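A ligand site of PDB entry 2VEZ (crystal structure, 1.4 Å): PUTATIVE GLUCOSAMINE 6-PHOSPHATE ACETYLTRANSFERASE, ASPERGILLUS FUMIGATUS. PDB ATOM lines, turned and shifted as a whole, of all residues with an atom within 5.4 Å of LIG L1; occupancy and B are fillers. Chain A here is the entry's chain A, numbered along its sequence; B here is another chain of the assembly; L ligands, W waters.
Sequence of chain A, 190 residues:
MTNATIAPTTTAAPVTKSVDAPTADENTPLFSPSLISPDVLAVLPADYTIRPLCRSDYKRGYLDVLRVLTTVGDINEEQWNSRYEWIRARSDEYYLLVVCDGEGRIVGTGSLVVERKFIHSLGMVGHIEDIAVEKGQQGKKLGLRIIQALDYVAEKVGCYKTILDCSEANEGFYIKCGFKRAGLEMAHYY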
ATOM      1  N   LEU A  69     -11.206   4.754  17.230  1.00  0.00           N
ATOM      2  CA  LEU A  69     -10.788   3.624  16.409  1.00  0.00           C
ATOM      3  C   LEU A  69     -10.579   4.112  15.008  1.00  0.00           C
ATOM      4  O   LEU A  69      -9.530   3.863  14.390  1.00  0.00           O
ATOM      5  CB  LEU A  69     -11.841   2.492  16.443  1.00  0.00           C
ATOM      6  CG  LEU A  69     -11.413   1.019  16.299  1.00  0.00           C
ATOM      7  CD1 LEU A  69     -12.586   0.243  15.688  1.00  0.00           C
ATOM      8  CD2 LEU A  69     -10.102   0.721  15.544  1.00  0.00           C
ATOM      9  N   THR A  70     -11.553   4.845  14.484  1.00  0.00           N
ATOM     10  CA  THR A  70     -11.560   5.145  13.054  1.00  0.00           C
ATOM     11  C   THR A  70     -12.706   6.107  12.848  1.00  0.00           C
ATOM     12  O   THR A  70     -13.350   6.544  13.821  1.00  0.00           O
ATOM     13  CB  THR A  70     -11.706   3.813  12.230  1.00  0.00           C
ATOM     14  OG1 THR A  70     -11.516   4.054  10.833  1.00  0.00           O
ATOM     15  CG2 THR A  70     -13.052   3.207  12.455  1.00  0.00           C
ATOM     16  N   THR A  71     -12.987   6.510  11.615  1.00  0.00           N
ATOM     17  CA  THR A  71     -14.051   7.495  11.550  1.00  0.00           C
ATOM     18  C   THR A  71     -15.450   6.939  11.457  1.00  0.00           C
ATOM     19  O   THR A  71     -15.690   5.848  10.930  1.00  0.00           O
ATOM     20  CB  THR A  71     -13.755   8.773  10.743  1.00  0.00           C
ATOM     21  OG1 THR A  71     -14.172   9.884  11.557  1.00  0.00           O
ATOM     22  CG2 THR A  71     -14.507   8.788   9.420  1.00  0.00           C
ATOM     23  N   ILE A 128     -13.789 -10.906  16.250  1.00  0.00           N
ATOM     24  CA  ILE A 128     -13.796  -9.750  17.151  1.00  0.00           C
ATOM     25  C   ILE A 128     -13.571  -8.487  16.311  1.00  0.00           C
ATOM     26  O   ILE A 128     -12.705  -8.450  15.430  1.00  0.00           O
ATOM     27  CB  ILE A 128     -12.765  -9.920  18.280  1.00  0.00           C
ATOM     28  CG1 ILE A 128     -13.333 -10.880  19.334  1.00  0.00           C
ATOM     29  CG2 ILE A 128     -12.358  -8.542  18.871  1.00  0.00           C
ATOM     30  CD1 ILE A 128     -12.357 -11.221  20.452  1.00  0.00           C
ATOM     31  N   GLU A 129     -14.407  -7.479  16.546  1.00  0.00           N
ATOM     32  CA  GLU A 129     -14.437  -6.261  15.749  1.00  0.00           C
ATOM     33  C   GLU A 129     -14.593  -5.019  16.612  1.00  0.00           C
ATOM     34  O   GLU A 129     -15.223  -5.049  17.684  1.00  0.00           O
ATOM     35  CB  GLU A 129     -15.650  -6.250  14.799  1.00  0.00           C
ATOM     36  CG  GLU A 129     -15.769  -7.456  13.889  1.00  0.00           C
ATOM     37  CD  GLU A 129     -14.756  -7.469  12.750  1.00  0.00           C
ATOM     38  OE1 GLU A 129     -14.093  -6.432  12.465  1.00  0.00           O
ATOM     39  OE2 GLU A 129     -14.669  -8.543  12.094  1.00  0.00           O
ATOM     40  N   ASP A 130     -14.042  -3.919  16.112  1.00  0.00           N
ATOM     41  CA  ASP A 130     -14.406  -2.606  16.621  1.00  0.00           C
ATOM     42  C   ASP A 130     -14.208  -2.438  18.121  1.00  0.00           C
ATOM     43  O   ASP A 130     -15.111  -1.983  18.851  1.00  0.00           O
ATOM     44  CB  ASP A 130     -15.836  -2.246  16.189  1.00  0.00           C
ATOM     45  CG  ASP A 130     -15.997  -2.277  14.669  1.00  0.00           C
ATOM     46  OD1 ASP A 130     -14.981  -2.056  13.998  1.00  0.00           O
ATOM     47  OD2 ASP A 130     -17.125  -2.516  14.170  1.00  0.00           O
ATOM     48  N   ILE A 131     -12.982  -2.759  18.545  1.00  0.00           N
ATOM     49  CA  ILE A 131     -12.560  -2.654  19.938  1.00  0.00           C
ATOM     50  C   ILE A 131     -12.026  -1.248  20.162  1.00  0.00           C
ATOM     51  O   ILE A 131     -11.131  -0.812  19.453  1.00  0.00           O
ATOM     52  CB  ILE A 131     -11.427  -3.668  20.233  1.00  0.00           C
ATOM     53  CG1 ILE A 131     -11.875  -5.082  19.864  1.00  0.00           C
ATOM     54  CG2 ILE A 131     -10.989  -3.609  21.704  1.00  0.00           C
ATOM     55  CD1 ILE A 131     -13.136  -5.576  20.596  1.00  0.00           C
ATOM     56  N   LEU A 164      -9.285 -12.098  14.815  1.00  0.00           N
ATOM     57  CA  LEU A 164      -9.418 -10.671  14.599  1.00  0.00           C
ATOM     58  C   LEU A 164      -8.207 -10.210  13.764  1.00  0.00           C
ATOM     59  O   LEU A 164      -7.212 -10.931  13.626  1.00  0.00           O
ATOM     60  CB  LEU A 164      -9.486  -9.927  15.957  1.00  0.00           C
ATOM     61  CG  LEU A 164      -8.285 -10.149  16.869  1.00  0.00           C
ATOM     62  CD1 LEU A 164      -7.160  -9.083  16.672  1.00  0.00           C
ATOM     63  CD2 LEU A 164      -8.700 -10.207  18.362  1.00  0.00           C
ATOM     64  N   ASP A 165      -8.299  -9.007  13.218  1.00  0.00           N
ATOM     65  CA  ASP A 165      -7.159  -8.356  12.588  1.00  0.00           C
ATOM     66  C   ASP A 165      -6.698  -7.180  13.415  1.00  0.00           C
ATOM     67  O   ASP A 165      -7.505  -6.491  14.038  1.00  0.00           O
ATOM     68  CB  ASP A 165      -7.552  -7.887  11.194  1.00  0.00           C
ATOM     69  CG  ASP A 165      -7.898  -9.031  10.265  1.00  0.00           C
ATOM     70  OD1 ASP A 165      -7.160 -10.022  10.178  1.00  0.00           O
ATOM     71  OD2 ASP A 165      -8.930  -8.921   9.633  1.00  0.00           O
ATOM     72  N   CYS A 166      -5.393  -6.956  13.403  1.00  0.00           N
ATOM     73  CA  CYS A 166      -4.838  -5.841  14.152  1.00  0.00           C
ATOM     74  C   CYS A 166      -3.657  -5.233  13.410  1.00  0.00           C
ATOM     75  O   CYS A 166      -3.233  -5.708  12.342  1.00  0.00           O
ATOM     76  CB  CYS A 166      -4.458  -6.276  15.569  1.00  0.00           C
ATOM     77  SG  CYS A 166      -3.004  -7.344  15.658  1.00  0.00           S
ATOM     78  N   SER A 167      -3.148  -4.132  13.936  1.00  0.00           N
ATOM     79  CA  SER A 167      -1.955  -3.488  13.373  1.00  0.00           C
ATOM     80  C   SER A 167      -0.696  -4.009  14.025  1.00  0.00           C
ATOM     81  O   SER A 167      -0.723  -4.601  15.117  1.00  0.00           O
ATOM     82  CB  SER A 167      -2.035  -1.966  13.576  1.00  0.00           C
ATOM     83  OG  SER A 167      -1.913  -1.649  14.962  1.00  0.00           O
ATOM     84  N   GLU A 185      -3.671  -9.999   7.189  1.00  0.00           N
ATOM     85  CA  GLU A 185      -4.867  -9.352   6.681  1.00  0.00           C
ATOM     86  C   GLU A 185      -4.582  -8.690   5.344  1.00  0.00           C
ATOM     87  O   GLU A 185      -3.619  -7.922   5.237  1.00  0.00           O
ATOM     88  CB  GLU A 185      -5.368  -8.275   7.637  1.00  0.00           C
ATOM     89  CG  GLU A 185      -6.693  -7.642   7.174  1.00  0.00           C
ATOM     90  CD  GLU A 185      -7.027  -6.359   7.903  1.00  0.00           C
ATOM     91  OE1 GLU A 185      -6.247  -5.932   8.770  1.00  0.00           O
ATOM     92  OE2 GLU A 185      -8.066  -5.749   7.543  1.00  0.00           O
ATOM     93  N   TYR A 189      -9.859  -1.688  -0.841  1.00  0.00           N
ATOM     94  CA  TYR A 189     -10.767  -0.544  -0.589  1.00  0.00           C
ATOM     95  C   TYR A 189     -11.361  -0.032  -1.904  1.00  0.00           C
ATOM     96  O   TYR A 189     -10.640   0.125  -2.896  1.00  0.00           O
ATOM     97  CB  TYR A 189     -10.015   0.605   0.139  1.00  0.00           C
ATOM     98  CG  TYR A 189      -9.802   0.380   1.614  1.00  0.00           C
ATOM     99  CD1 TYR A 189     -10.569   1.056   2.568  1.00  0.00           C
ATOM    100  CD2 TYR A 189      -8.836  -0.513   2.074  1.00  0.00           C
ATOM    101  CE1 TYR A 189     -10.380   0.842   3.942  1.00  0.00           C
ATOM    102  CE2 TYR A 189      -8.647  -0.740   3.423  1.00  0.00           C
ATOM    103  CZ  TYR A 189      -9.405  -0.056   4.358  1.00  0.00           C
ATOM    104  OH  TYR A 189      -9.194  -0.309   5.697  1.00  0.00           O
ATOM    105  N   LYS B 117     -21.538  -2.464  10.264  1.00  0.00           N
ATOM    106  CA  LYS B 117     -20.838  -1.664  11.259  1.00  0.00           C
ATOM    107  C   LYS B 117     -21.623  -0.394  11.640  1.00  0.00           C
ATOM    108  O   LYS B 117     -22.575  -0.059  10.983  1.00  0.00           O
ATOM    109  CB  LYS B 117     -19.440  -1.269  10.792  1.00  0.00           C
ATOM    110  CG  LYS B 117     -18.434  -2.456  10.657  1.00  0.00           C
ATOM    111  CD  LYS B 117     -17.034  -1.969  10.547  1.00  0.00           C
ATOM    112  CE  LYS B 117     -16.027  -3.143  10.501  1.00  0.00           C
ATOM    113  NZ  LYS B 117     -16.096  -4.040  11.643  1.00  0.00           N
ATOM    114  N   ILE B 119     -19.348   2.292  12.463  1.00  0.00           N
ATOM    115  CA  ILE B 119     -18.305   3.141  11.882  1.00  0.00           C
ATOM    116  C   ILE B 119     -18.494   3.318  10.369  1.00  0.00           C
ATOM    117  O   ILE B 119     -19.272   2.605   9.724  1.00  0.00           O
ATOM    118  CB  ILE B 119     -16.864   2.624  12.187  1.00  0.00           C
ATOM    119  CG1 ILE B 119     -16.661   1.256  11.521  1.00  0.00           C
ATOM    120  CG2 ILE B 119     -16.653   2.542  13.709  1.00  0.00           C
ATOM    121  CD1 ILE B 119     -15.263   0.676  11.533  1.00  0.00           C
ATOM    122  N   HIS B 120     -17.836   4.336   9.824  1.00  0.00           N
ATOM    123  CA  HIS B 120     -17.936   4.666   8.378  1.00  0.00           C
ATOM    124  C   HIS B 120     -19.380   4.960   7.979  1.00  0.00           C
ATOM    125  O   HIS B 120     -19.878   4.467   6.936  1.00  0.00           O
ATOM    126  CB  HIS B 120     -17.378   3.526   7.493  1.00  0.00           C
ATOM    127  CG  HIS B 120     -15.892   3.433   7.524  1.00  0.00           C
ATOM    128  ND1 HIS B 120     -15.089   3.909   6.517  1.00  0.00           N
ATOM    129  CD2 HIS B 120     -15.064   2.882   8.444  1.00  0.00           C
ATOM    130  CE1 HIS B 120     -13.826   3.693   6.827  1.00  0.00           C
ATOM    131  NE2 HIS B 120     -13.788   3.063   7.987  1.00  0.00           N
ATOM    132  N   VAL B 125     -18.672  -4.018   5.521  1.00  0.00           N
ATOM    133  CA  VAL B 125     -17.377  -4.578   5.134  1.00  0.00           C
ATOM    134  C   VAL B 125     -17.600  -5.975   4.578  1.00  0.00           C
ATOM    135  O   VAL B 125     -18.295  -6.781   5.174  1.00  0.00           O
ATOM    136  CB  VAL B 125     -16.425  -4.632   6.338  1.00  0.00           C
ATOM    137  CG1 VAL B 125     -15.132  -5.393   5.979  1.00  0.00           C
ATOM    138  CG2 VAL B 125     -16.087  -3.203   6.792  1.00  0.00           C
ATOM    139  N   TYR B 160     -17.616  -0.711   1.724  1.00  0.00           N
ATOM    140  CA  TYR B 160     -16.544   0.254   1.465  1.00  0.00           C
ATOM    141  C   TYR B 160     -15.186  -0.409   1.241  1.00  0.00           C
ATOM    142  O   TYR B 160     -14.252   0.211   0.717  1.00  0.00           O
ATOM    143  CB  TYR B 160     -16.469   1.332   2.557  1.00  0.00           C
ATOM    144  CG  TYR B 160     -16.068   0.877   3.944  1.00  0.00           C
ATOM    145  CD1 TYR B 160     -14.719   0.847   4.320  1.00  0.00           C
ATOM    146  CD2 TYR B 160     -17.016   0.553   4.904  1.00  0.00           C
ATOM    147  CE1 TYR B 160     -14.327   0.473   5.619  1.00  0.00           C
ATOM    148  CE2 TYR B 160     -16.644   0.165   6.210  1.00  0.00           C
ATOM    149  CZ  TYR B 160     -15.285   0.126   6.551  1.00  0.00           C
ATOM    150  OH  TYR B 160     -14.902  -0.264   7.835  1.00  0.00           O
ATOM    151  N   LYS B 161     -15.093  -1.671   1.650  1.00  0.00           N
ATOM    152  CA  LYS B 161     -13.877  -2.439   1.389  1.00  0.00           C
ATOM    153  C   LYS B 161     -14.235  -3.912   1.502  1.00  0.00           C
ATOM    154  O   LYS B 161     -15.283  -4.263   2.047  1.00  0.00           O
ATOM    155  CB  LYS B 161     -12.775  -2.082   2.414  1.00  0.00           C
ATOM    156  CG  LYS B 161     -13.097  -2.526   3.847  1.00  0.00           C
ATOM    157  CD  LYS B 161     -11.981  -2.222   4.844  1.00  0.00           C
ATOM    158  CE  LYS B 161     -12.312  -2.816   6.186  1.00  0.00           C
ATOM    159  NZ  LYS B 161     -11.292  -2.432   7.235  1.00  0.00           N
HETATM  160  C1  LIG L   1      -9.234  -3.292  12.297  1.00  0.00           C
HETATM  161  C2  LIG L   1     -10.155  -4.045  13.250  1.00  0.00           C
HETATM  162  C3  LIG L   1     -11.623  -3.953  12.785  1.00  0.00           C
HETATM  163  C4  LIG L   1     -12.068  -2.522  12.547  1.00  0.00           C
HETATM  164  C5  LIG L   1     -11.069  -1.860  11.600  1.00  0.00           C
HETATM  165  C6  LIG L   1     -11.466  -0.415  11.332  1.00  0.00           C
HETATM  166  O1  LIG L   1      -7.879  -3.369  12.752  1.00  0.00           O
HETATM  167  O2  LIG L   1      -9.822  -5.409  13.264  1.00  0.00           O
HETATM  168  O3  LIG L   1     -12.428  -4.521  13.783  1.00  0.00           O
HETATM  169  O4  LIG L   1     -13.347  -2.565  11.931  1.00  0.00           O
HETATM  170  O5  LIG L   1      -9.723  -1.910  12.161  1.00  0.00           O
HETATM  171  O6  LIG L   1     -10.566   0.123  10.382  1.00  0.00           O
HETATM  172  P1  LIG L   1     -11.160   0.704   8.985  1.00  0.00           P
HETATM  173  O7  LIG L   1      -9.961   1.165   8.055  1.00  0.00           O
HETATM  174  O8  LIG L   1     -11.894   2.077   9.355  1.00  0.00           O
HETATM  175  O9  LIG L   1     -12.154  -0.183   8.305  1.00  0.00           O
HETATM  176  N1  LG2 L   2       0.967  -2.409  22.467  1.00  0.00           N
HETATM  177  C1  LG2 L   2       1.462  -3.125  23.488  1.00  0.00           C
HETATM  178  N2  LG2 L   2       0.824  -3.257  24.674  1.00  0.00           N
HETATM  179  C2  LG2 L   2      -0.370  -2.646  24.871  1.00  0.00           C
HETATM  180  C3  LG2 L   2      -0.964  -1.830  23.815  1.00  0.00           C
HETATM  181  C4  LG2 L   2      -0.214  -1.739  22.557  1.00  0.00           C
HETATM  182  N3  LG2 L   2      -0.711  -1.000  21.533  1.00  0.00           N
HETATM  183  N4  LG2 L   2      -2.131  -1.328  24.281  1.00  0.00           N
HETATM  184  C5  LG2 L   2      -2.263  -1.808  25.554  1.00  0.00           C
HETATM  185  N5  LG2 L   2      -1.211  -2.573  25.904  1.00  0.00           N
HETATM  186  C6  LG2 L   2      -0.978  -3.319  27.173  1.00  0.00           C
HETATM  187  C7  LG2 L   2      -1.398  -2.603  28.437  1.00  0.00           C
HETATM  188  O1  LG2 L   2      -0.374  -1.668  28.857  1.00  0.00           O
HETATM  189  C8  LG2 L   2      -1.586  -3.805  29.358  1.00  0.00           C
HETATM  190  O2  LG2 L   2      -0.312  -4.353  29.715  1.00  0.00           O
HETATM  191  P1  LG2 L   2       0.047  -5.000  31.157  1.00  0.00           P
HETATM  192  O3  LG2 L   2      -0.656  -6.323  31.245  1.00  0.00           O
HETATM  193  O4  LG2 L   2       1.554  -5.126  31.134  1.00  0.00           O
HETATM  194  O5  LG2 L   2      -0.557  -3.918  32.015  1.00  0.00           O
HETATM  195  C9  LG2 L   2      -2.262  -4.848  28.460  1.00  0.00           C
HETATM  196  O6  LG2 L   2      -1.797  -4.513  27.131  1.00  0.00           O
HETATM  197  C10 LG2 L   2      -3.787  -4.749  28.465  1.00  0.00           C
HETATM  198  O7  LG2 L   2      -4.176  -3.474  27.950  1.00  0.00           O
HETATM  199  P2  LG2 L   2      -5.441  -2.645  28.456  1.00  0.00           P
HETATM  200  O8  LG2 L   2      -5.048  -1.827  29.643  1.00  0.00           O
HETATM  201  O9  LG2 L   2      -6.601  -3.564  28.588  1.00  0.00           O
HETATM  202  O10 LG2 L   2      -5.502  -1.689  27.173  1.00  0.00           O
HETATM  203  P3  LG2 L   2      -6.630  -0.652  26.748  1.00  0.00           P
HETATM  204  O11 LG2 L   2      -5.951   0.625  26.383  1.00  0.00           O
HETATM  205  O12 LG2 L   2      -7.772  -0.600  27.739  1.00  0.00           O
HETATM  206  O13 LG2 L   2      -7.203  -1.212  25.350  1.00  0.00           O
HETATM  207  C11 LG2 L   2      -6.934  -0.797  23.014  1.00  0.00           C
HETATM  208  C12 LG2 L   2      -6.338  -1.460  24.248  1.00  0.00           C
HETATM  209  C13 LG2 L   2      -8.304  -1.407  22.712  1.00  0.00           C
HETATM  210  C14 LG2 L   2      -5.986  -1.092  21.849  1.00  0.00           C
HETATM  211  C15 LG2 L   2      -7.074   0.730  23.222  1.00  0.00           C
HETATM  212  O14 LG2 L   2      -5.805   1.277  23.626  1.00  0.00           O
HETATM  213  C16 LG2 L   2      -7.656   1.490  22.052  1.00  0.00           C
HETATM  214  O15 LG2 L   2      -8.862   1.694  21.978  1.00  0.00           O
HETATM  215  N6  LG2 L   2      -6.800   1.948  21.110  1.00  0.00           N
HETATM  216  C17 LG2 L   2      -7.212   2.704  19.928  1.00  0.00           C
HETATM  217  C18 LG2 L   2      -8.132   1.910  18.990  1.00  0.00           C
HETATM  218  C19 LG2 L   2      -7.566   0.538  18.703  1.00  0.00           C
HETATM  219  O16 LG2 L   2      -6.388   0.399  18.357  1.00  0.00           O
HETATM  220  N7  LG2 L   2      -8.415  -0.490  18.823  1.00  0.00           N
HETATM  221  C20 LG2 L   2      -8.094  -1.851  18.448  1.00  0.00           C
HETATM  222  C21 LG2 L   2      -8.376  -2.084  16.963  1.00  0.00           C
HETATM  223  S1  LG2 L   2      -8.158  -3.784  16.503  1.00  0.00           S
HETATM  224  C22 LG2 L   2      -9.703  -4.449  16.604  1.00  0.00           C
HETATM  225  O17 LG2 L   2     -10.713  -3.748  16.831  1.00  0.00           O
HETATM  226  C23 LG2 L   2      -9.845  -5.940  16.476  1.00  0.00           C
HETATM  227  O   HOH W   1      -9.943  -4.986   9.961  1.00  0.00           O
HETATM  228  O   HOH W   2     -10.871  -7.197  10.685  1.00  0.00           O
HETATM  229  O   HOH W   3     -10.883  -7.631  13.517  1.00  0.00           O
HETATM  230  O   HOH W   4     -12.444  -3.629   9.268  1.00  0.00           O
HETATM  231  O   HOH W   5      -5.726  -2.311  14.772  1.00  0.00           O
HETATM  232  O   HOH W   6      -8.075   0.275  12.283  1.00  0.00           O
HETATM  233  O   HOH W   7      -6.393  -3.951  10.553  1.00  0.00           O
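An oxygen (O8) of LIG L1 sits at hydrogen-bond distance from the side-chain hydroxyl of Thr 70. A ring nitrogen (NE2) of His 120 of chain B is in hydrogen-bond range of an oxygen (O8) of LIG L1 (2.5 Å). The side-chain amino group of Lys 161 of chain B is in salt-bridge range of an oxygen (O9) of LIG L1 (2.6 Å). An oxygen (O2) of LIG L1 sits at hydrogen-bond distance from the backbone carbonyl oxygen (O) of Asp 165, at 2.7 Å. N of Asp 130 sits at hydrogen-bond distance from O3 of LIG L1 (2.9 Å). The side-chain carboxylate (OD1) of Asp 130 lies within hydrogen-bond range of an oxygen (O4) of LIG L1 (2.7 Å). An oxygen (O9) of LIG L1 is in hydrogen-bond range of the side-chain hydroxyl of Tyr 160 of chain B, at 2.8 Å. OE1 of Glu 129 is in hydrogen-bond range of O3 of LIG L1 (2.9 Å). The side-chain hydroxyl (OH) of Tyr 189 lies within hydrogen-bond range of an oxygen (O7) of LIG L1 (2.9 Å). O4 of LIG L1 lies close to NZ of Lys 117 of chain B, 3.1 Å away. O17 of LG2 L2 lies within hydrogen-bond range of N of Asp 130, at 3.4 Å. N of Ile 131 sits at hydrogen-bond distance from O17 of LG2 L2 (3.0 Å). A nitrogen (N7) of LG2 L2 sits at hydrogen-bond distance from the backbone carbonyl oxygen (O) of Ile 131, at 2.8 Å.
O1 of LIG L1 sits close to S1 of LG2 L2, at 3.8 Å.
The backbone carbonyl oxygen of Thr 71 lies within hydrogen-bond range of the backbone NH of His 120 of chain B. OH of Tyr 189 sits at hydrogen-bond distance from NZ of Lys 161 of chain B, 3.4 Å away. The side-chain amino group (NZ) of Lys 117 of chain B is in salt-bridge range of the side-chain carboxylate (OD2) of Asp 130, 3.1 Å away. The side-chain amino group (NZ) of Lys 117 of chain B lies within salt-bridge range of the side-chain carboxylate (OE1) of Glu 129.
Ile 119 of chain B touches LIG L1 (CD1 to O4, 3.8 Å). Of the 19 residues printed, 10 come within 4 Å of LIG L1.
Water W3 lies within hydrogen-bond range of an oxygen (O2) of LIG L1 (2.5 Å), the backbone carbonyl oxygen (O) of Ile 128 (2.8 Å) and the backbone NH (N) of Asp 165 (2.9 Å). Water W7 bridges OE1 of Glu 185 (2.7 Å) and O1 of LIG L1 (2.7 Å). Water W1 lies within hydrogen-bond range of OE2 of Glu 185 (3.2 Å) and O2 of LIG L1 (3.3 Å). Water W4 bridges the side-chain amino group (NZ) of Lys 161 of chain B (2.6 Å) and an oxygen (O4) of LIG L1 (3.0 Å). Water W5 lies within hydrogen-bond range of an oxygen (O1) of LIG L1 (3.1 Å), the backbone NH of Ser 167 (3.3 Å) and a sulfur (S1) of LG2 L2 (3.3 Å). Water W2 bridges OD2 of Asp 165 (2.8 Å) and O2 of LIG L1 (3.3 Å).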
